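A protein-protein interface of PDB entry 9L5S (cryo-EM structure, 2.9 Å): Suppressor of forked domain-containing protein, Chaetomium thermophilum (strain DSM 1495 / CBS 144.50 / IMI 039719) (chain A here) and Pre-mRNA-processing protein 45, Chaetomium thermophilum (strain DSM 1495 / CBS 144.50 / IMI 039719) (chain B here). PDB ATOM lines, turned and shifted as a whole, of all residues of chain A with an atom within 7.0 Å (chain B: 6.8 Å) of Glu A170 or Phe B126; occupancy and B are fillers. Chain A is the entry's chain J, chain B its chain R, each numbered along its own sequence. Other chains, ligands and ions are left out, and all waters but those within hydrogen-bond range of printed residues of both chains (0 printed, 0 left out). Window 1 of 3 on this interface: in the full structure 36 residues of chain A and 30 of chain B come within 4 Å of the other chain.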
ATOM      1  N   ARG A 138       8.042 -19.327  19.612  1.00  0.00           N
ATOM      2  CA  ARG A 138       7.761 -20.387  20.570  1.00  0.00           C
ATOM      3  C   ARG A 138       6.418 -21.057  20.322  1.00  0.00           C
ATOM      4  O   ARG A 138       5.983 -21.874  21.141  1.00  0.00           O
ATOM      5  CB  ARG A 138       7.828 -19.843  21.998  1.00  0.00           C
ATOM      6  CG  ARG A 138       9.213 -19.382  22.388  1.00  0.00           C
ATOM      7  CD  ARG A 138      10.156 -20.560  22.473  1.00  0.00           C
ATOM      8  NE  ARG A 138      11.291 -20.304  23.347  1.00  0.00           N
ATOM      9  CZ  ARG A 138      12.269 -21.169  23.567  1.00  0.00           C
ATOM     10  NH1 ARG A 138      12.285 -22.355  22.984  1.00  0.00           N
ATOM     11  NH2 ARG A 138      13.258 -20.834  24.386  1.00  0.00           N
ATOM     12  N   ASP A 164      16.913 -25.734  10.710  1.00  0.00           N
ATOM     13  CA  ASP A 164      18.110 -25.234  11.380  1.00  0.00           C
ATOM     14  C   ASP A 164      17.803 -24.004  12.225  1.00  0.00           C
ATOM     15  O   ASP A 164      18.321 -23.865  13.337  1.00  0.00           O
ATOM     16  CB  ASP A 164      19.197 -24.921  10.352  1.00  0.00           C
ATOM     17  CG  ASP A 164      20.135 -26.089  10.122  1.00  0.00           C
ATOM     18  OD1 ASP A 164      20.528 -26.742  11.111  1.00  0.00           O
ATOM     19  OD2 ASP A 164      20.485 -26.352   8.952  1.00  0.00           O
ATOM     20  N   ARG A 165      16.959 -23.104  11.713  1.00  0.00           N
ATOM     21  CA  ARG A 165      16.514 -21.962  12.511  1.00  0.00           C
ATOM     22  C   ARG A 165      15.713 -22.419  13.729  1.00  0.00           C
ATOM     23  O   ARG A 165      15.898 -21.907  14.847  1.00  0.00           O
ATOM     24  CB  ARG A 165      15.675 -21.024  11.646  1.00  0.00           C
ATOM     25  CG  ARG A 165      16.434 -20.390  10.499  1.00  0.00           C
ATOM     26  CD  ARG A 165      15.491 -20.007   9.373  1.00  0.00           C
ATOM     27  NE  ARG A 165      14.526 -18.996   9.785  1.00  0.00           N
ATOM     28  CZ  ARG A 165      13.526 -18.564   9.030  1.00  0.00           C
ATOM     29  NH1 ARG A 165      13.322 -19.040   7.814  1.00  0.00           N
ATOM     30  NH2 ARG A 165      12.709 -17.630   9.508  1.00  0.00           N
ATOM     31  N   TRP A 166      14.825 -23.396  13.525  1.00  0.00           N
ATOM     32  CA  TRP A 166      14.029 -23.933  14.625  1.00  0.00           C
ATOM     33  C   TRP A 166      14.921 -24.560  15.689  1.00  0.00           C
ATOM     34  O   TRP A 166      14.712 -24.344  16.887  1.00  0.00           O
ATOM     35  CB  TRP A 166      13.024 -24.952  14.087  1.00  0.00           C
ATOM     36  CG  TRP A 166      11.870 -25.237  15.004  1.00  0.00           C
ATOM     37  CD1 TRP A 166      11.644 -24.697  16.235  1.00  0.00           C
ATOM     38  CD2 TRP A 166      10.774 -26.123  14.748  1.00  0.00           C
ATOM     39  NE1 TRP A 166      10.480 -25.194  16.764  1.00  0.00           N
ATOM     40  CE2 TRP A 166       9.927 -26.075  15.872  1.00  0.00           C
ATOM     41  CE3 TRP A 166      10.428 -26.955  13.679  1.00  0.00           C
ATOM     42  CZ2 TRP A 166       8.754 -26.821  15.956  1.00  0.00           C
ATOM     43  CZ3 TRP A 166       9.267 -27.698  13.767  1.00  0.00           C
ATOM     44  CH2 TRP A 166       8.444 -27.626  14.897  1.00  0.00           C
ATOM     45  N   MET A 167      15.941 -25.312  15.269  1.00  0.00           N
ATOM     46  CA  MET A 167      16.875 -25.914  16.210  1.00  0.00           C
ATOM     47  C   MET A 167      17.765 -24.873  16.873  1.00  0.00           C
ATOM     48  O   MET A 167      18.245 -25.108  17.987  1.00  0.00           O
ATOM     49  CB  MET A 167      17.745 -26.957  15.510  1.00  0.00           C
ATOM     50  CG  MET A 167      16.999 -28.208  15.085  1.00  0.00           C
ATOM     51  SD  MET A 167      15.706 -28.717  16.225  1.00  0.00           S
ATOM     52  CE  MET A 167      14.255 -28.459  15.211  1.00  0.00           C
ATOM     53  N   LYS A 168      18.013 -23.743  16.202  1.00  0.00           N
ATOM     54  CA  LYS A 168      18.657 -22.616  16.865  1.00  0.00           C
ATOM     55  C   LYS A 168      17.802 -22.095  18.006  1.00  0.00           C
ATOM     56  O   LYS A 168      18.334 -21.668  19.037  1.00  0.00           O
ATOM     57  CB  LYS A 168      18.936 -21.484  15.876  1.00  0.00           C
ATOM     58  CG  LYS A 168      20.225 -21.610  15.089  1.00  0.00           C
ATOM     59  CD  LYS A 168      20.559 -20.295  14.395  1.00  0.00           C
ATOM     60  CE  LYS A 168      19.449 -19.855  13.452  1.00  0.00           C
ATOM     61  NZ  LYS A 168      19.744 -18.546  12.807  1.00  0.00           N
ATOM     62  N   TRP A 169      16.479 -22.127  17.850  1.00  0.00           N
ATOM     63  CA  TRP A 169      15.603 -21.703  18.940  1.00  0.00           C
ATOM     64  C   TRP A 169      15.447 -22.737  20.054  1.00  0.00           C
ATOM     65  O   TRP A 169      14.716 -22.464  21.014  1.00  0.00           O
ATOM     66  CB  TRP A 169      14.225 -21.316  18.398  1.00  0.00           C
ATOM     67  CG  TRP A 169      14.179 -19.893  17.966  1.00  0.00           C
ATOM     68  CD1 TRP A 169      14.331 -19.410  16.703  1.00  0.00           C
ATOM     69  CD2 TRP A 169      14.005 -18.755  18.815  1.00  0.00           C
ATOM     70  NE1 TRP A 169      14.244 -18.039  16.707  1.00  0.00           N
ATOM     71  CE2 TRP A 169      14.047 -17.613  17.994  1.00  0.00           C
ATOM     72  CE3 TRP A 169      13.810 -18.591  20.189  1.00  0.00           C
ATOM     73  CZ2 TRP A 169      13.896 -16.325  18.502  1.00  0.00           C
ATOM     74  CZ3 TRP A 169      13.664 -17.316  20.691  1.00  0.00           C
ATOM     75  CH2 TRP A 169      13.708 -16.198  19.849  1.00  0.00           C
ATOM     76  N   GLU A 170      16.126 -23.882  19.963  1.00  0.00           N
ATOM     77  CA  GLU A 170      16.106 -24.932  20.978  1.00  0.00           C
ATOM     78  C   GLU A 170      14.700 -25.401  21.363  1.00  0.00           C
ATOM     79  O   GLU A 170      14.237 -25.141  22.480  1.00  0.00           O
ATOM     80  CB  GLU A 170      16.883 -24.502  22.215  1.00  0.00           C
ATOM     81  CG  GLU A 170      18.369 -24.316  21.980  1.00  0.00           C
ATOM     82  CD  GLU A 170      19.160 -24.293  23.271  1.00  0.00           C
ATOM     83  OE1 GLU A 170      18.588 -24.641  24.324  1.00  0.00           O
ATOM     84  OE2 GLU A 170      20.351 -23.919  23.235  1.00  0.00           O
ATOM     85  N   PRO A 171      14.000 -26.091  20.468  1.00  0.00           N
ATOM     86  CA  PRO A 171      12.606 -26.462  20.741  1.00  0.00           C
ATOM     87  C   PRO A 171      12.484 -27.714  21.592  1.00  0.00           C
ATOM     88  O   PRO A 171      13.480 -28.231  22.106  1.00  0.00           O
ATOM     89  CB  PRO A 171      12.039 -26.691  19.340  1.00  0.00           C
ATOM     90  CG  PRO A 171      13.214 -27.197  18.572  1.00  0.00           C
ATOM     91  CD  PRO A 171      14.453 -26.595  19.161  1.00  0.00           C
ATOM     92  N   ASP A 172      11.256 -28.207  21.745  1.00  0.00           N
ATOM     93  CA  ASP A 172      11.020 -29.461  22.439  1.00  0.00           C
ATOM     94  C   ASP A 172      11.510 -30.642  21.598  1.00  0.00           C
ATOM     95  O   ASP A 172      11.936 -30.492  20.450  1.00  0.00           O
ATOM     96  CB  ASP A 172       9.536 -29.623  22.766  1.00  0.00           C
ATOM     97  CG  ASP A 172       9.096 -28.757  23.930  1.00  0.00           C
ATOM     98  OD1 ASP A 172       9.968 -28.299  24.697  1.00  0.00           O
ATOM     99  OD2 ASP A 172       7.876 -28.534  24.078  1.00  0.00           O
ATOM    100  N   TRP A 176      12.932 -31.948  17.199  1.00  0.00           N
ATOM    101  CA  TRP A 176      14.156 -32.689  16.914  1.00  0.00           C
ATOM    102  C   TRP A 176      13.847 -34.026  16.255  1.00  0.00           C
ATOM    103  O   TRP A 176      14.507 -34.412  15.284  1.00  0.00           O
ATOM    104  CB  TRP A 176      14.963 -32.903  18.194  1.00  0.00           C
ATOM    105  CG  TRP A 176      15.497 -31.644  18.797  1.00  0.00           C
ATOM    106  CD1 TRP A 176      14.900 -30.870  19.745  1.00  0.00           C
ATOM    107  CD2 TRP A 176      16.748 -31.018  18.497  1.00  0.00           C
ATOM    108  NE1 TRP A 176      15.698 -29.795  20.049  1.00  0.00           N
ATOM    109  CE2 TRP A 176      16.838 -29.863  19.294  1.00  0.00           C
ATOM    110  CE3 TRP A 176      17.794 -31.318  17.620  1.00  0.00           C
ATOM    111  CZ2 TRP A 176      17.935 -29.009  19.245  1.00  0.00           C
ATOM    112  CZ3 TRP A 176      18.883 -30.470  17.575  1.00  0.00           C
ATOM    113  CH2 TRP A 176      18.947 -29.330  18.384  1.00  0.00           C
ATOM    114  N   GLN A 201      23.007 -32.525  23.092  1.00  0.00           N
ATOM    115  CA  GLN A 201      23.426 -31.324  23.809  1.00  0.00           C
ATOM    116  C   GLN A 201      22.222 -30.564  24.361  1.00  0.00           C
ATOM    117  O   GLN A 201      22.226 -30.128  25.517  1.00  0.00           O
ATOM    118  CB  GLN A 201      24.268 -30.429  22.901  1.00  0.00           C
ATOM    119  CG  GLN A 201      25.609 -31.037  22.530  1.00  0.00           C
ATOM    120  CD  GLN A 201      26.415 -30.156  21.598  1.00  0.00           C
ATOM    121  OE1 GLN A 201      26.009 -29.042  21.272  1.00  0.00           O
ATOM    122  NE2 GLN A 201      27.563 -30.657  21.159  1.00  0.00           N
ATOM    123  N   VAL A 202      21.176 -30.402  23.547  1.00  0.00           N
ATOM    124  CA  VAL A 202      20.014 -29.616  23.956  1.00  0.00           C
ATOM    125  C   VAL A 202      19.151 -30.397  24.944  1.00  0.00           C
ATOM    126  O   VAL A 202      18.757 -29.874  25.993  1.00  0.00           O
ATOM    127  CB  VAL A 202      19.210 -29.178  22.719  1.00  0.00           C
ATOM    128  CG1 VAL A 202      17.794 -28.775  23.095  1.00  0.00           C
ATOM    129  CG2 VAL A 202      19.911 -28.027  22.040  1.00  0.00           C
ATOM    130  N   HIS A 203      18.846 -31.652  24.624  1.00  0.00           N
ATOM    131  CA  HIS A 203      17.992 -32.497  25.452  1.00  0.00           C
ATOM    132  C   HIS A 203      18.798 -33.648  26.036  1.00  0.00           C
ATOM    133  O   HIS A 203      18.721 -34.775  25.533  1.00  0.00           O
ATOM    134  CB  HIS A 203      16.822 -33.044  24.629  1.00  0.00           C
ATOM    135  CG  HIS A 203      15.804 -32.012  24.265  1.00  0.00           C
ATOM    136  ND1 HIS A 203      15.027 -31.373  25.204  1.00  0.00           N
ATOM    137  CD2 HIS A 203      15.447 -31.494  23.067  1.00  0.00           C
ATOM    138  CE1 HIS A 203      14.227 -30.513  24.600  1.00  0.00           C
ATOM    139  NE2 HIS A 203      14.462 -30.566  23.303  1.00  0.00           N
ATOM    140  N   ALA B 124      15.329 -10.583  19.436  1.00  0.00           N
ATOM    141  CA  ALA B 124      14.805 -11.371  18.328  1.00  0.00           C
ATOM    142  C   ALA B 124      15.483 -12.725  18.159  1.00  0.00           C
ATOM    143  O   ALA B 124      15.238 -13.394  17.147  1.00  0.00           O
ATOM    144  CB  ALA B 124      14.912 -10.582  17.019  1.00  0.00           C
ATOM    145  N   SER B 125      16.321 -13.156  19.098  1.00  0.00           N
ATOM    146  CA  SER B 125      16.995 -14.441  18.987  1.00  0.00           C
ATOM    147  C   SER B 125      16.990 -15.134  20.340  1.00  0.00           C
ATOM    148  O   SER B 125      16.733 -14.518  21.377  1.00  0.00           O
ATOM    149  CB  SER B 125      18.429 -14.283  18.470  1.00  0.00           C
ATOM    150  OG  SER B 125      19.274 -13.747  19.472  1.00  0.00           O
ATOM    151  N   PHE B 126      17.299 -16.434  20.320  1.00  0.00           N
ATOM    152  CA  PHE B 126      17.371 -17.226  21.545  1.00  0.00           C
ATOM    153  C   PHE B 126      18.483 -16.754  22.473  1.00  0.00           C
ATOM    154  O   PHE B 126      18.406 -16.987  23.685  1.00  0.00           O
ATOM    155  CB  PHE B 126      17.560 -18.706  21.188  1.00  0.00           C
ATOM    156  CG  PHE B 126      17.637 -19.620  22.380  1.00  0.00           C
ATOM    157  CD1 PHE B 126      16.490 -20.001  23.054  1.00  0.00           C
ATOM    158  CD2 PHE B 126      18.859 -20.103  22.819  1.00  0.00           C
ATOM    159  CE1 PHE B 126      16.561 -20.840  24.152  1.00  0.00           C
ATOM    160  CE2 PHE B 126      18.936 -20.940  23.914  1.00  0.00           C
ATOM    161  CZ  PHE B 126      17.786 -21.310  24.579  1.00  0.00           C
ATOM    162  N   LYS B 127      19.498 -16.079  21.929  1.00  0.00           N
ATOM    163  CA  LYS B 127      20.597 -15.550  22.731  1.00  0.00           C
ATOM    164  C   LYS B 127      20.116 -14.517  23.749  1.00  0.00           C
ATOM    165  O   LYS B 127      20.747 -14.338  24.796  1.00  0.00           O
ATOM    166  CB  LYS B 127      21.653 -14.959  21.793  1.00  0.00           C
ATOM    167  CG  LYS B 127      22.990 -14.611  22.419  1.00  0.00           C
ATOM    168  CD  LYS B 127      23.105 -13.116  22.658  1.00  0.00           C
ATOM    169  CE  LYS B 127      23.032 -12.340  21.354  1.00  0.00           C
ATOM    170  NZ  LYS B 127      23.072 -10.870  21.583  1.00  0.00           N
ATOM    171  N   ASP B 128      18.999 -13.840  23.468  1.00  0.00           N
ATOM    172  CA  ASP B 128      18.413 -12.910  24.424  1.00  0.00           C
ATOM    173  C   ASP B 128      17.714 -13.608  25.585  1.00  0.00           C
ATOM    174  O   ASP B 128      17.445 -12.958  26.601  1.00  0.00           O
ATOM    175  CB  ASP B 128      17.424 -11.986  23.714  1.00  0.00           C
ATOM    176  CG  ASP B 128      18.083 -11.139  22.649  1.00  0.00           C
ATOM    177  OD1 ASP B 128      18.973 -10.336  22.995  1.00  0.00           O
ATOM    178  OD2 ASP B 128      17.717 -11.280  21.464  1.00  0.00           O
ATOM    179  N   LEU B 129      17.411 -14.898  25.465  1.00  0.00           N
ATOM    180  CA  LEU B 129      16.774 -15.647  26.540  1.00  0.00           C
ATOM    181  C   LEU B 129      17.772 -16.242  27.523  1.00  0.00           C
ATOM    182  O   LEU B 129      17.357 -16.847  28.515  1.00  0.00           O
ATOM    183  CB  LEU B 129      15.900 -16.764  25.964  1.00  0.00           C
ATOM    184  CG  LEU B 129      14.796 -16.325  25.005  1.00  0.00           C
ATOM    185  CD1 LEU B 129      13.958 -17.513  24.586  1.00  0.00           C
ATOM    186  CD2 LEU B 129      13.926 -15.272  25.660  1.00  0.00           C
ATOM    187  N   ILE B 130      19.066 -16.085  27.273  1.00  0.00           N
ATOM    188  CA  ILE B 130      20.102 -16.630  28.144  1.00  0.00           C
ATOM    189  C   ILE B 130      20.491 -15.547  29.145  1.00  0.00           C
ATOM    190  O   ILE B 130      20.495 -14.359  28.790  1.00  0.00           O
ATOM    191  CB  ILE B 130      21.303 -17.124  27.318  1.00  0.00           C
ATOM    192  CG1 ILE B 130      20.828 -18.132  26.271  1.00  0.00           C
ATOM    193  CG2 ILE B 130      22.367 -17.764  28.196  1.00  0.00           C
ATOM    194  CD1 ILE B 130      21.933 -18.702  25.426  1.00  0.00           C
ATOM    195  N   MET B 240       8.950 -13.266  23.250  1.00  0.00           N
ATOM    196  CA  MET B 240      10.097 -14.010  23.768  1.00  0.00           C
ATOM    197  C   MET B 240       9.713 -14.859  24.980  1.00  0.00           C
ATOM    198  O   MET B 240      10.314 -14.759  26.046  1.00  0.00           O
ATOM    199  CB  MET B 240      11.218 -13.038  24.117  1.00  0.00           C
ATOM    200  CG  MET B 240      11.582 -12.105  22.981  1.00  0.00           C
ATOM    201  SD  MET B 240      12.296 -12.986  21.589  1.00  0.00           S
ATOM    202  CE  MET B 240      13.814 -13.543  22.340  1.00  0.00           C
ATOM    203  N   PRO B 243       9.432 -21.916  26.812  1.00  0.00           N
ATOM    204  CA  PRO B 243       8.631 -22.983  26.214  1.00  0.00           C
ATOM    205  C   PRO B 243       7.382 -23.250  27.029  1.00  0.00           C
ATOM    206  O   PRO B 243       7.392 -23.141  28.270  1.00  0.00           O
ATOM    207  CB  PRO B 243       9.582 -24.186  26.226  1.00  0.00           C
ATOM    208  CG  PRO B 243      10.920 -23.582  26.163  1.00  0.00           C
ATOM    209  CD  PRO B 243      10.832 -22.345  26.991  1.00  0.00           C
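Among the printed residues, merely in contact across the chains: Arg A138 with Phe B126, Arg A138 with Leu B129, Arg A138 with Pro B243, Lys A168 with Phe B126, Trp A169 with Ala B124, Trp A169 with Ser B125, Trp A169 with Phe B126, Trp A169 with Leu B129, Trp A169 with Met B240 and Glu A170 with Phe B126.
NH1 of Arg A138 sits at hydrogen-bond distance from O of Trp A169 (3.1 Å).
The guanidinium group of Arg A138 lies within hydrogen-bond range of the backbone carbonyl oxygen of Glu A170.
The side-chain carboxylate (OD2) of Asp B128 sits at hydrogen-bond distance from the backbone NH (N) of Ala B124 (3.2 Å).
N of Lys B127 lies close to OG of Ser B125 (3.4 Å).
OD2 of Asp B128 lies within hydrogen-bond range of N of Ser B125, 3.3 Å away.
Glu A170 touches just one residue of chain B: Phe B126.
Phe B126 touches just these residues of chain A: Arg A138, Lys A168, Trp A169 and Glu A170.
Printed residues of chain A within 4 Å of Met B240: Trp A169 (3.6 Å).
Of the printed residues of chain B, Trp A169 touches Ala B124, Ser B125, Phe B126, Leu B129 and Met B240.
Arg A165 touches none of the printed residues of chain B.
The nearest residue of chain A that does not touch Phe B126 is Pro A171 (6.9 Å).
Printed residues of chain B that touch a printed residue of chain A: Ala B124, Ser B125, Phe B126, Leu B129, Met B240 and Pro B243.
Hydrophobic or aromatic side chains of chain B within 4 Å of the printed part of chain A: Phe B126, Leu B129, Met B240 and Pro B243.
Of the 14 printed residues of chain A, 4 touch a printed residue of chain B.
Printed residues of chain A that touch a printed residue of chain B: Arg A138, Lys A168, Trp A169 and Glu A170.
Hydrophobic or aromatic side chains of chain A that line the printed part of chain B: Trp A169.
Among the printed residues, no Asp or Glu carboxylate lies within 4 Å of a Lys or Arg side-chain nitrogen of the other chain.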
